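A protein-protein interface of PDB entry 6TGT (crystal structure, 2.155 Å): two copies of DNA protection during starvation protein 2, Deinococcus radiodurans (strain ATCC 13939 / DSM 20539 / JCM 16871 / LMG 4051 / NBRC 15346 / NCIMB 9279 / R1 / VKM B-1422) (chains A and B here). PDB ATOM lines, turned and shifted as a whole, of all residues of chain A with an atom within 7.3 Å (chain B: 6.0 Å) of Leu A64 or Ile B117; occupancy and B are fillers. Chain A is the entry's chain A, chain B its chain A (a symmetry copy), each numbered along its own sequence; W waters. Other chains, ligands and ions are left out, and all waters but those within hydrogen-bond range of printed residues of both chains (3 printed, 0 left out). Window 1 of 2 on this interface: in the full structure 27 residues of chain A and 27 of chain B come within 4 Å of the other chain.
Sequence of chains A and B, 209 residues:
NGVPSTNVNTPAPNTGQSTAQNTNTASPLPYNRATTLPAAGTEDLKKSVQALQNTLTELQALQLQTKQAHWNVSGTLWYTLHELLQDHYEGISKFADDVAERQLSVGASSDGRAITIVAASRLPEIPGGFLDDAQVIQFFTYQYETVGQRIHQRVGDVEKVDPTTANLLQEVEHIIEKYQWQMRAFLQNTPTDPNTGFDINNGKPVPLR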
ATOM      1  N   GLU A  58     -10.024  12.522 -27.577  1.00  0.00           N
ATOM      2  CA  GLU A  58      -9.338  12.449 -28.862  1.00  0.00           C
ATOM      3  C   GLU A  58      -8.220  13.480 -28.949  1.00  0.00           C
ATOM      4  O   GLU A  58      -7.147  13.194 -29.492  1.00  0.00           O
ATOM      5  CB  GLU A  58     -10.338  12.640 -30.003  1.00  0.00           C
ATOM      6  CG  GLU A  58     -11.363  11.524 -30.116  1.00  0.00           C
ATOM      7  CD  GLU A  58     -12.532  11.893 -31.006  1.00  0.00           C
ATOM      8  OE1 GLU A  58     -12.637  13.075 -31.394  1.00  0.00           O
ATOM      9  OE2 GLU A  58     -13.348  10.999 -31.317  1.00  0.00           O
ATOM     10  N   LEU A  59      -8.453  14.684 -28.419  1.00  0.00           N
ATOM     11  CA  LEU A  59      -7.407  15.702 -28.411  1.00  0.00           C
ATOM     12  C   LEU A  59      -6.240  15.282 -27.528  1.00  0.00           C
ATOM     13  O   LEU A  59      -5.075  15.471 -27.898  1.00  0.00           O
ATOM     14  CB  LEU A  59      -7.981  17.040 -27.945  1.00  0.00           C
ATOM     15  CG  LEU A  59      -8.963  17.722 -28.899  1.00  0.00           C
ATOM     16  CD1 LEU A  59      -9.515  19.001 -28.287  1.00  0.00           C
ATOM     17  CD2 LEU A  59      -8.304  18.005 -30.240  1.00  0.00           C
ATOM     18  N   GLN A  60      -6.531  14.707 -26.359  1.00  0.00           N
ATOM     19  CA  GLN A  60      -5.465  14.231 -25.485  1.00  0.00           C
ATOM     20  C   GLN A  60      -4.697  13.076 -26.114  1.00  0.00           C
ATOM     21  O   GLN A  60      -3.486  12.947 -25.895  1.00  0.00           O
ATOM     22  CB  GLN A  60      -6.045  13.807 -24.138  1.00  0.00           C
ATOM     23  CG  GLN A  60      -6.357  14.964 -23.209  1.00  0.00           C
ATOM     24  CD  GLN A  60      -6.910  14.496 -21.882  1.00  0.00           C
ATOM     25  OE1 GLN A  60      -7.875  13.735 -21.836  1.00  0.00           O
ATOM     26  NE2 GLN A  60      -6.298  14.943 -20.793  1.00  0.00           N
ATOM     27  N   ALA A  61      -5.377  12.228 -26.889  1.00  0.00           N
ATOM     28  CA  ALA A  61      -4.682  11.165 -27.605  1.00  0.00           C
ATOM     29  C   ALA A  61      -3.746  11.743 -28.658  1.00  0.00           C
ATOM     30  O   ALA A  61      -2.585  11.333 -28.766  1.00  0.00           O
ATOM     31  CB  ALA A  61      -5.691  10.209 -28.240  1.00  0.00           C
ATOM     32  N   LEU A  62      -4.238  12.704 -29.446  1.00  0.00           N
ATOM     33  CA  LEU A  62      -3.383  13.377 -30.418  1.00  0.00           C
ATOM     34  C   LEU A  62      -2.272  14.159 -29.732  1.00  0.00           C
ATOM     35  O   LEU A  62      -1.171  14.282 -30.280  1.00  0.00           O
ATOM     36  CB  LEU A  62      -4.220  14.303 -31.300  1.00  0.00           C
ATOM     37  CG  LEU A  62      -5.229  13.622 -32.227  1.00  0.00           C
ATOM     38  CD1 LEU A  62      -6.108  14.653 -32.917  1.00  0.00           C
ATOM     39  CD2 LEU A  62      -4.516  12.749 -33.247  1.00  0.00           C
ATOM     40  N   GLN A  63      -2.547  14.692 -28.538  1.00  0.00           N
ATOM     41  CA  GLN A  63      -1.522  15.381 -27.760  1.00  0.00           C
ATOM     42  C   GLN A  63      -0.306  14.490 -27.539  1.00  0.00           C
ATOM     43  O   GLN A  63       0.827  14.868 -27.855  1.00  0.00           O
ATOM     44  CB  GLN A  63      -2.107  15.822 -26.417  1.00  0.00           C
ATOM     45  CG  GLN A  63      -1.960  17.295 -26.100  1.00  0.00           C
ATOM     46  CD  GLN A  63      -2.524  17.640 -24.736  1.00  0.00           C
ATOM     47  OE1 GLN A  63      -3.406  16.950 -24.223  1.00  0.00           O
ATOM     48  NE2 GLN A  63      -2.011  18.705 -24.135  1.00  0.00           N
ATOM     49  N   LEU A  64      -0.530  13.290 -26.998  1.00  0.00           N
ATOM     50  CA  LEU A  64       0.577  12.385 -26.710  1.00  0.00           C
ATOM     51  C   LEU A  64       1.174  11.797 -27.982  1.00  0.00           C
ATOM     52  O   LEU A  64       2.358  11.445 -28.001  1.00  0.00           O
ATOM     53  CB  LEU A  64       0.110  11.269 -25.777  1.00  0.00           C
ATOM     54  CG  LEU A  64      -0.239  11.696 -24.350  1.00  0.00           C
ATOM     55  CD1 LEU A  64      -1.077  10.633 -23.661  1.00  0.00           C
ATOM     56  CD2 LEU A  64       1.022  11.985 -23.554  1.00  0.00           C
ATOM     57  N   GLN A  65       0.379  11.682 -29.049  1.00  0.00           N
ATOM     58  CA  GLN A  65       0.880  11.085 -30.282  1.00  0.00           C
ATOM     59  C   GLN A  65       1.721  12.067 -31.089  1.00  0.00           C
ATOM     60  O   GLN A  65       2.765  11.689 -31.633  1.00  0.00           O
ATOM     61  CB  GLN A  65      -0.285  10.559 -31.121  1.00  0.00           C
ATOM     62  CG  GLN A  65      -0.881   9.262 -30.595  1.00  0.00           C
ATOM     63  CD  GLN A  65      -2.181   8.893 -31.280  1.00  0.00           C
ATOM     64  OE1 GLN A  65      -2.651   9.604 -32.168  1.00  0.00           O
ATOM     65  NE2 GLN A  65      -2.772   7.777 -30.869  1.00  0.00           N
ATOM     66  N   THR A  66       1.286  13.327 -31.183  1.00  0.00           N
ATOM     67  CA  THR A  66       2.098  14.331 -31.863  1.00  0.00           C
ATOM     68  C   THR A  66       3.431  14.521 -31.154  1.00  0.00           C
ATOM     69  O   THR A  66       4.479  14.627 -31.801  1.00  0.00           O
ATOM     70  CB  THR A  66       1.350  15.664 -31.948  1.00  0.00           C
ATOM     71  OG1 THR A  66       0.887  16.042 -30.646  1.00  0.00           O
ATOM     72  CG2 THR A  66       0.166  15.557 -32.897  1.00  0.00           C
ATOM     73  N   LYS A  67       3.411  14.559 -29.820  1.00  0.00           N
ATOM     74  CA  LYS A  67       4.649  14.722 -29.065  1.00  0.00           C
ATOM     75  C   LYS A  67       5.539  13.491 -29.187  1.00  0.00           C
ATOM     76  O   LYS A  67       6.769  13.611 -29.234  1.00  0.00           O
ATOM     77  CB  LYS A  67       4.327  15.016 -27.601  1.00  0.00           C
ATOM     78  CG  LYS A  67       5.542  15.313 -26.748  1.00  0.00           C
ATOM     79  CD  LYS A  67       6.120  16.684 -27.057  1.00  0.00           C
ATOM     80  CE  LYS A  67       5.291  17.786 -26.421  1.00  0.00           C
ATOM     81  NZ  LYS A  67       6.065  19.049 -26.273  1.00  0.00           N
ATOM     82  N   GLN A  68       4.937  12.300 -29.240  1.00  0.00           N
ATOM     83  CA  GLN A  68       5.719  11.080 -29.413  1.00  0.00           C
ATOM     84  C   GLN A  68       6.438  11.081 -30.756  1.00  0.00           C
ATOM     85  O   GLN A  68       7.643  10.810 -30.828  1.00  0.00           O
ATOM     86  CB  GLN A  68       4.816   9.852 -29.286  1.00  0.00           C
ATOM     87  CG  GLN A  68       5.497   8.537 -29.633  1.00  0.00           C
ATOM     88  CD  GLN A  68       6.388   8.029 -28.516  1.00  0.00           C
ATOM     89  OE1 GLN A  68       6.417   8.593 -27.422  1.00  0.00           O
ATOM     90  NE2 GLN A  68       7.120   6.954 -28.787  1.00  0.00           N
ATOM     91  N   ALA A  69       5.711  11.383 -31.833  1.00  0.00           N
ATOM     92  CA  ALA A  69       6.346  11.505 -33.140  1.00  0.00           C
ATOM     93  C   ALA A  69       7.297  12.693 -33.189  1.00  0.00           C
ATOM     94  O   ALA A  69       8.285  12.665 -33.928  1.00  0.00           O
ATOM     95  CB  ALA A  69       5.283  11.627 -34.230  1.00  0.00           C
ATOM     96  N   HIS A  70       7.013  13.737 -32.406  1.00  0.00           N
ATOM     97  CA  HIS A  70       7.890  14.904 -32.352  1.00  0.00           C
ATOM     98  C   HIS A  70       9.299  14.521 -31.911  1.00  0.00           C
ATOM     99  O   HIS A  70      10.286  15.081 -32.403  1.00  0.00           O
ATOM    100  CB  HIS A  70       7.285  15.946 -31.409  1.00  0.00           C
ATOM    101  CG  HIS A  70       8.222  17.048 -31.019  1.00  0.00           C
ATOM    102  ND1 HIS A  70       8.432  18.159 -31.805  1.00  0.00           N
ATOM    103  CD2 HIS A  70       8.982  17.219 -29.913  1.00  0.00           C
ATOM    104  CE1 HIS A  70       9.289  18.965 -31.204  1.00  0.00           C
ATOM    105  NE2 HIS A  70       9.640  18.416 -30.054  1.00  0.00           N
ATOM    106  N   TYR A  89       1.037  20.215 -31.650  1.00  0.00           N
ATOM    107  CA  TYR A  89       0.864  19.906 -30.234  1.00  0.00           C
ATOM    108  C   TYR A  89       0.350  21.113 -29.461  1.00  0.00           C
ATOM    109  O   TYR A  89      -0.535  20.982 -28.607  1.00  0.00           O
ATOM    110  CB  TYR A  89       2.186  19.416 -29.642  1.00  0.00           C
ATOM    111  CG  TYR A  89       2.129  19.158 -28.153  1.00  0.00           C
ATOM    112  CD1 TYR A  89       1.655  17.951 -27.658  1.00  0.00           C
ATOM    113  CD2 TYR A  89       2.548  20.120 -27.243  1.00  0.00           C
ATOM    114  CE1 TYR A  89       1.598  17.709 -26.300  1.00  0.00           C
ATOM    115  CE2 TYR A  89       2.494  19.889 -25.882  1.00  0.00           C
ATOM    116  CZ  TYR A  89       2.019  18.681 -25.416  1.00  0.00           C
ATOM    117  OH  TYR A  89       1.962  18.441 -24.063  1.00  0.00           O
ATOM    118  N   ILE A  92      -3.315  21.745 -30.419  1.00  0.00           N
ATOM    119  CA  ILE A  92      -4.172  20.713 -29.845  1.00  0.00           C
ATOM    120  C   ILE A  92      -4.300  20.899 -28.337  1.00  0.00           C
ATOM    121  O   ILE A  92      -5.395  20.781 -27.774  1.00  0.00           O
ATOM    122  CB  ILE A  92      -3.630  19.315 -30.202  1.00  0.00           C
ATOM    123  CG1 ILE A  92      -3.829  19.024 -31.691  1.00  0.00           C
ATOM    124  CG2 ILE A  92      -4.296  18.243 -29.351  1.00  0.00           C
ATOM    125  CD1 ILE A  92      -2.983  17.872 -32.201  1.00  0.00           C
ATOM    126  N   SER A  93      -3.186  21.201 -27.663  1.00  0.00           N
ATOM    127  CA  SER A  93      -3.215  21.371 -26.213  1.00  0.00           C
ATOM    128  C   SER A  93      -4.088  22.552 -25.809  1.00  0.00           C
ATOM    129  O   SER A  93      -4.813  22.485 -24.810  1.00  0.00           O
ATOM    130  CB  SER A  93      -1.796  21.556 -25.677  1.00  0.00           C
ATOM    131  OG  SER A  93      -0.974  20.443 -25.989  1.00  0.00           O
ATOM    132  N   ALA A 114      -5.217   9.480 -17.612  1.00  0.00           N
ATOM    133  CA  ALA A 114      -4.495   8.617 -18.540  1.00  0.00           C
ATOM    134  C   ALA A 114      -5.293   7.361 -18.867  1.00  0.00           C
ATOM    135  O   ALA A 114      -5.325   6.921 -20.023  1.00  0.00           O
ATOM    136  CB  ALA A 114      -3.131   8.246 -17.959  1.00  0.00           C
ATOM    137  N   ILE A 115      -5.941   6.768 -17.861  1.00  0.00           N
ATOM    138  CA  ILE A 115      -6.725   5.560 -18.104  1.00  0.00           C
ATOM    139  C   ILE A 115      -7.882   5.850 -19.050  1.00  0.00           C
ATOM    140  O   ILE A 115      -8.242   5.005 -19.877  1.00  0.00           O
ATOM    141  CB  ILE A 115      -7.211   4.957 -16.767  1.00  0.00           C
ATOM    142  CG1 ILE A 115      -7.959   3.648 -17.013  1.00  0.00           C
ATOM    143  CG2 ILE A 115      -8.081   5.945 -16.000  1.00  0.00           C
ATOM    144  CD1 ILE A 115      -7.115   2.582 -17.677  1.00  0.00           C
ATOM    145  N   ILE A 117      -7.892   8.027 -21.511  1.00  0.00           N
ATOM    146  CA  ILE A 117      -7.347   8.108 -22.863  1.00  0.00           C
ATOM    147  C   ILE A 117      -7.205   6.714 -23.459  1.00  0.00           C
ATOM    148  O   ILE A 117      -7.539   6.484 -24.629  1.00  0.00           O
ATOM    149  CB  ILE A 117      -6.002   8.858 -22.852  1.00  0.00           C
ATOM    150  CG1 ILE A 117      -6.188  10.285 -22.332  1.00  0.00           C
ATOM    151  CG2 ILE A 117      -5.385   8.869 -24.244  1.00  0.00           C
ATOM    152  CD1 ILE A 117      -4.887  11.010 -22.060  1.00  0.00           C
ATOM    153  N   VAL A 118      -6.719   5.760 -22.663  1.00  0.00           N
ATOM    154  CA  VAL A 118      -6.570   4.393 -23.147  1.00  0.00           C
ATOM    155  C   VAL A 118      -7.926   3.704 -23.238  1.00  0.00           C
ATOM    156  O   VAL A 118      -8.218   3.008 -24.217  1.00  0.00           O
ATOM    157  CB  VAL A 118      -5.594   3.615 -22.246  1.00  0.00           C
ATOM    158  CG1 VAL A 118      -5.534   2.156 -22.663  1.00  0.00           C
ATOM    159  CG2 VAL A 118      -4.210   4.244 -22.300  1.00  0.00           C
ATOM    160  N   GLU A 125      -3.157   3.380 -31.845  1.00  0.00           N
ATOM    161  CA  GLU A 125      -2.035   3.929 -31.101  1.00  0.00           C
ATOM    162  C   GLU A 125      -0.824   4.072 -32.012  1.00  0.00           C
ATOM    163  O   GLU A 125      -0.566   3.214 -32.861  1.00  0.00           O
ATOM    164  CB  GLU A 125      -1.694   3.038 -29.905  1.00  0.00           C
ATOM    165  CG  GLU A 125      -0.480   3.488 -29.103  1.00  0.00           C
ATOM    166  CD  GLU A 125      -0.725   4.775 -28.338  1.00  0.00           C
ATOM    167  OE1 GLU A 125      -1.164   4.701 -27.171  1.00  0.00           O
ATOM    168  OE2 GLU A 125      -0.478   5.862 -28.903  1.00  0.00           O
ATOM    169  N   ILE A 126      -0.095   5.167 -31.839  1.00  0.00           N
ATOM    170  CA  ILE A 126       1.114   5.403 -32.637  1.00  0.00           C
ATOM    171  C   ILE A 126       2.157   4.347 -32.287  1.00  0.00           C
ATOM    172  O   ILE A 126       2.264   3.954 -31.110  1.00  0.00           O
ATOM    173  CB  ILE A 126       1.641   6.824 -32.390  1.00  0.00           C
ATOM    174  CG1 ILE A 126       2.731   7.194 -33.399  1.00  0.00           C
ATOM    175  CG2 ILE A 126       2.136   6.996 -30.955  1.00  0.00           C
ATOM    176  CD1 ILE A 126       2.864   8.684 -33.628  1.00  0.00           C
ATOM    177  N   PHE A 140      -0.770  10.587 -39.263  1.00  0.00           N
ATOM    178  CA  PHE A 140      -1.578  11.742 -38.898  1.00  0.00           C
ATOM    179  C   PHE A 140      -2.485  12.211 -40.028  1.00  0.00           C
ATOM    180  O   PHE A 140      -3.479  12.894 -39.759  1.00  0.00           O
ATOM    181  CB  PHE A 140      -0.676  12.885 -38.432  1.00  0.00           C
ATOM    182  CG  PHE A 140      -0.066  12.652 -37.082  1.00  0.00           C
ATOM    183  CD1 PHE A 140      -0.836  12.760 -35.935  1.00  0.00           C
ATOM    184  CD2 PHE A 140       1.269  12.308 -36.958  1.00  0.00           C
ATOM    185  CE1 PHE A 140      -0.281  12.539 -34.688  1.00  0.00           C
ATOM    186  CE2 PHE A 140       1.829  12.087 -35.715  1.00  0.00           C
ATOM    187  CZ  PHE A 140       1.055  12.203 -34.578  1.00  0.00           C
ATOM    188  N   THR B  57       7.923   8.798 -17.743  1.00  0.00           N
ATOM    189  CA  THR B  57       6.579   8.271 -17.527  1.00  0.00           C
ATOM    190  C   THR B  57       5.949   8.867 -16.273  1.00  0.00           C
ATOM    191  O   THR B  57       4.753   9.179 -16.258  1.00  0.00           O
ATOM    192  CB  THR B  57       6.624   6.745 -17.439  1.00  0.00           C
ATOM    193  OG1 THR B  57       7.177   6.215 -18.651  1.00  0.00           O
ATOM    194  CG2 THR B  57       5.228   6.175 -17.237  1.00  0.00           C
ATOM    195  N   GLN B  60       4.938  12.423 -17.154  1.00  0.00           N
ATOM    196  CA  GLN B  60       3.727  12.418 -17.966  1.00  0.00           C
ATOM    197  C   GLN B  60       2.499  12.059 -17.140  1.00  0.00           C
ATOM    198  O   GLN B  60       1.403  12.566 -17.408  1.00  0.00           O
ATOM    199  CB  GLN B  60       3.883  11.446 -19.132  1.00  0.00           C
ATOM    200  CG  GLN B  60       4.710  11.987 -20.281  1.00  0.00           C
ATOM    201  CD  GLN B  60       4.821  10.997 -21.418  1.00  0.00           C
ATOM    202  OE1 GLN B  60       5.206   9.847 -21.216  1.00  0.00           O
ATOM    203  NE2 GLN B  60       4.478  11.436 -22.623  1.00  0.00           N
ATOM    204  N   ALA B  61       2.657  11.187 -16.142  1.00  0.00           N
ATOM    205  CA  ALA B  61       1.546  10.881 -15.248  1.00  0.00           C
ATOM    206  C   ALA B  61       1.157  12.105 -14.428  1.00  0.00           C
ATOM    207  O   ALA B  61      -0.028  12.435 -14.311  1.00  0.00           O
ATOM    208  CB  ALA B  61       1.911   9.709 -14.336  1.00  0.00           C
ATOM    209  N   GLN B  63       1.763  15.102 -15.322  1.00  0.00           N
ATOM    210  CA  GLN B  63       1.230  16.034 -16.310  1.00  0.00           C
ATOM    211  C   GLN B  63      -0.288  15.931 -16.402  1.00  0.00           C
ATOM    212  O   GLN B  63      -1.004  16.930 -16.265  1.00  0.00           O
ATOM    213  CB  GLN B  63       1.863  15.754 -17.674  1.00  0.00           C
ATOM    214  CG  GLN B  63       2.524  16.943 -18.337  1.00  0.00           C
ATOM    215  CD  GLN B  63       3.087  16.592 -19.701  1.00  0.00           C
ATOM    216  OE1 GLN B  63       3.407  15.435 -19.973  1.00  0.00           O
ATOM    217  NE2 GLN B  63       3.199  17.588 -20.569  1.00  0.00           N
ATOM    218  N   LEU B  64      -0.796  14.719 -16.629  1.00  0.00           N
ATOM    219  CA  LEU B  64      -2.235  14.530 -16.775  1.00  0.00           C
ATOM    220  C   LEU B  64      -2.964  14.681 -15.447  1.00  0.00           C
ATOM    221  O   LEU B  64      -4.143  15.051 -15.430  1.00  0.00           O
ATOM    222  CB  LEU B  64      -2.523  13.158 -17.385  1.00  0.00           C
ATOM    223  CG  LEU B  64      -2.099  12.976 -18.843  1.00  0.00           C
ATOM    224  CD1 LEU B  64      -2.031  11.502 -19.203  1.00  0.00           C
ATOM    225  CD2 LEU B  64      -3.050  13.712 -19.773  1.00  0.00           C
ATOM    226  N   GLY B 112       6.615   7.834 -24.850  1.00  0.00           N
ATOM    227  CA  GLY B 112       5.710   8.680 -24.099  1.00  0.00           C
ATOM    228  C   GLY B 112       4.261   8.450 -24.470  1.00  0.00           C
ATOM    229  O   GLY B 112       3.424   9.348 -24.331  1.00  0.00           O
ATOM    230  N   ARG B 113       3.953   7.246 -24.942  1.00  0.00           N
ATOM    231  CA  ARG B 113       2.607   6.935 -25.397  1.00  0.00           C
ATOM    232  C   ARG B 113       1.659   6.766 -24.213  1.00  0.00           C
ATOM    233  O   ARG B 113       2.071   6.527 -23.075  1.00  0.00           O
ATOM    234  CB  ARG B 113       2.617   5.672 -26.258  1.00  0.00           C
ATOM    235  CG  ARG B 113       3.507   5.778 -27.487  1.00  0.00           C
ATOM    236  CD  ARG B 113       3.689   4.428 -28.159  1.00  0.00           C
ATOM    237  NE  ARG B 113       4.356   3.469 -27.283  1.00  0.00           N
ATOM    238  CZ  ARG B 113       4.191   2.153 -27.357  1.00  0.00           C
ATOM    239  NH1 ARG B 113       3.378   1.635 -28.268  1.00  0.00           N
ATOM    240  NH2 ARG B 113       4.839   1.353 -26.519  1.00  0.00           N
ATOM    241  N   ALA B 114       0.360   6.892 -24.504  1.00  0.00           N
ATOM    242  CA  ALA B 114      -0.648   6.812 -23.452  1.00  0.00           C
ATOM    243  C   ALA B 114      -0.646   5.442 -22.785  1.00  0.00           C
ATOM    244  O   ALA B 114      -0.778   5.342 -21.558  1.00  0.00           O
ATOM    245  CB  ALA B 114      -2.030   7.124 -24.026  1.00  0.00           C
ATOM    246  N   ILE B 115      -0.503   4.376 -23.574  1.00  0.00           N
ATOM    247  CA  ILE B 115      -0.492   3.033 -23.001  1.00  0.00           C
ATOM    248  C   ILE B 115       0.698   2.854 -22.069  1.00  0.00           C
ATOM    249  O   ILE B 115       0.595   2.172 -21.043  1.00  0.00           O
ATOM    250  CB  ILE B 115      -0.512   1.969 -24.120  1.00  0.00           C
ATOM    251  CG1 ILE B 115      -0.587   0.565 -23.522  1.00  0.00           C
ATOM    252  CG2 ILE B 115       0.700   2.107 -25.034  1.00  0.00           C
ATOM    253  CD1 ILE B 115      -1.827   0.326 -22.689  1.00  0.00           C
ATOM    254  N   THR B 116       1.833   3.481 -22.387  1.00  0.00           N
ATOM    255  CA  THR B 116       3.013   3.363 -21.536  1.00  0.00           C
ATOM    256  C   THR B 116       2.797   4.054 -20.196  1.00  0.00           C
ATOM    257  O   THR B 116       3.281   3.578 -19.160  1.00  0.00           O
ATOM    258  CB  THR B 116       4.233   3.943 -22.253  1.00  0.00           C
ATOM    259  OG1 THR B 116       4.388   3.298 -23.524  1.00  0.00           O
ATOM    260  CG2 THR B 116       5.494   3.731 -21.425  1.00  0.00           C
ATOM    261  N   ILE B 117       2.073   5.175 -20.193  1.00  0.00           N
ATOM    262  CA  ILE B 117       1.759   5.855 -18.939  1.00  0.00           C
ATOM    263  C   ILE B 117       0.921   4.952 -18.045  1.00  0.00           C
ATOM    264  O   ILE B 117       1.156   4.859 -16.833  1.00  0.00           O
ATOM    265  CB  ILE B 117       1.047   7.191 -19.221  1.00  0.00           C
ATOM    266  CG1 ILE B 117       1.947   8.114 -20.046  1.00  0.00           C
ATOM    267  CG2 ILE B 117       0.638   7.864 -17.918  1.00  0.00           C
ATOM    268  CD1 ILE B 117       1.239   9.345 -20.573  1.00  0.00           C
ATOM    269  N   VAL B 118      -0.064   4.265 -18.628  1.00  0.00           N
ATOM    270  CA  VAL B 118      -0.902   3.362 -17.848  1.00  0.00           C
ATOM    271  C   VAL B 118      -0.141   2.087 -17.502  1.00  0.00           C
ATOM    272  O   VAL B 118      -0.209   1.597 -16.369  1.00  0.00           O
ATOM    273  CB  VAL B 118      -2.205   3.060 -18.609  1.00  0.00           C
ATOM    274  CG1 VAL B 118      -3.025   2.018 -17.867  1.00  0.00           C
ATOM    275  CG2 VAL B 118      -3.012   4.335 -18.802  1.00  0.00           C
ATOM    276  N   ALA B 119       0.600   1.535 -18.466  1.00  0.00           N
ATOM    277  CA  ALA B 119       1.365   0.310 -18.251  1.00  0.00           C
ATOM    278  C   ALA B 119       2.403   0.495 -17.153  1.00  0.00           C
ATOM    279  O   ALA B 119       2.258  -0.054 -16.055  1.00  0.00           O
ATOM    280  CB  ALA B 119       2.052  -0.136 -19.543  1.00  0.00           C
ATOM    281  N   ALA B 120       3.452   1.265 -17.438  1.00  0.00           N
ATOM    282  CA  ALA B 120       4.503   1.544 -16.460  1.00  0.00           C
ATOM    283  C   ALA B 120       4.023   2.580 -15.440  1.00  0.00           C
ATOM    284  O   ALA B 120       4.619   3.638 -15.243  1.00  0.00           O
ATOM    285  CB  ALA B 120       5.770   2.003 -17.169  1.00  0.00           C
ATOM    286  N   SER B 121       2.913   2.248 -14.781  1.00  0.00           N
ATOM    287  CA  SER B 121       2.301   3.137 -13.802  1.00  0.00           C
ATOM    288  C   SER B 121       3.165   3.264 -12.554  1.00  0.00           C
ATOM    289  O   SER B 121       3.994   4.174 -12.455  1.00  0.00           O
ATOM    290  CB  SER B 121       0.904   2.634 -13.428  1.00  0.00           C
ATOM    291  OG  SER B 121       0.576   2.978 -12.095  1.00  0.00           O
HETATM  292  O   HOH W   1      -0.212   7.586 -27.079  1.00  0.00           O
HETATM  293  O   HOH W   2       3.959  11.852 -25.675  1.00  0.00           O
HETATM  294  O   HOH W   3      -5.421  15.709 -17.894  1.00  0.00           O
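The side-chain amide oxygen of Gln A68 is in hydrogen-bond range of the backbone NH of Gly B112 (2.7 Å).
The backbone carbonyl oxygen (O) of Tyr A89 is in hydrogen-bond range of the side-chain hydroxyl (OG) of Ser A93 (2.7 Å). The side-chain amide nitrogen (NE2) of Gln B60 lies within hydrogen-bond range of the backbone carbonyl oxygen (O) of Gly B112 (2.9 Å).
Among the printed residues, pairs that only touch across the chains: Gln A60 with Leu B64 (3.6 Å), Leu A64 with Gln B60 (3.6 Å), Leu A64 with Gly B112 (3.7 Å), Leu A64 with Ala B114 (3.7 Å), Leu A64 with Ile B117 (3.99 Å), Gln A68 with Arg B113 (3.7 Å), Tyr A89 with Gln B63 (3.8 Å), Ala A114 with Leu B64 (3.7 Å), Ala A114 with Ile B117 (3.8 Å), Ala A114 with Val B118 (3.7 Å), Ile A115 with Val B118 (3.9 Å), Ile A117 with Leu B64 (3.99 Å), Ile A117 with Ala B114 (3.8 Å), Val A118 with Ala B114 (3.7 Å), Val A118 with Ile B115 (3.9 Å), Val A118 with Val B118 (3.7 Å), Glu A125 with Ala B114 (3.8 Å), Glu A125 with Ile B115 (3.7 Å) and Ile A126 with Arg B113 (3.3 Å).
Printed residues of chain B within 4 Å of Leu A64: Gln B60, Gly B112, Ala B114 and Ile B117. Printed residues of chain A within 4 Å of Ile B117: Leu A64 and Ala A114. Of the printed residues of chain A, Gln B63 touches Tyr A89 (3.8 Å). Of the printed residues of chain A, Ala B114 touches Leu A64 (3.7 Å), Ile A117 (3.8 Å), Val A118 (3.7 Å) and Glu A125 (3.8 Å). Ala B61 touches none of the printed residues of chain A. The nearest printed residue of chain B that does not touch Leu A64 is Leu B64 (4.6 Å).
Hydrophobic or aromatic side chains of chain A within 4 Å of the printed part of chain B: Leu A64, Tyr A89, Ala A114, Ile A117, Val A118 and Ile A126. Along chain A the printed residues that touch a printed residue of chain B span positions 60 to 126. Printed residues of chain B that touch a printed residue of chain A: Gln B60, Gln B63, Leu B64, Gly B112, Arg B113, Ala B114, Ile B115, Ile B117 and Val B118. Among the printed residues, 20 pairs touch across the chains.
Leu A64 touches Ala B114, and with the chains exchanged Ala A114 touches Leu B64. Ala A114 touches Ile B117, and with the chains exchanged Ile A117 touches Ala B114. Ile A115 touches Val B118, and with the chains exchanged Val A118 touches Ile B115. Val A118 touches its own counterpart, Val B118. Positions printed for both chains: 60, 61, 63, 64, 114, 115, 117 and 118. Of the 20 pairs that touch across the chains among the printed residues, 13 have their exchanged pair printed and touching as well.
Water W1 bridges OE2 of Glu A125 and N of Ala B114. Water W2 lies within hydrogen-bond range of O of Leu A64 (2.9 Å), O of Gly B112 (2.9 Å) and NE2 of Gln B60 (3.1 Å). Water W3 bridges the backbone carbonyl oxygen of Leu B64 and the side-chain amide nitrogen of Gln A60.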
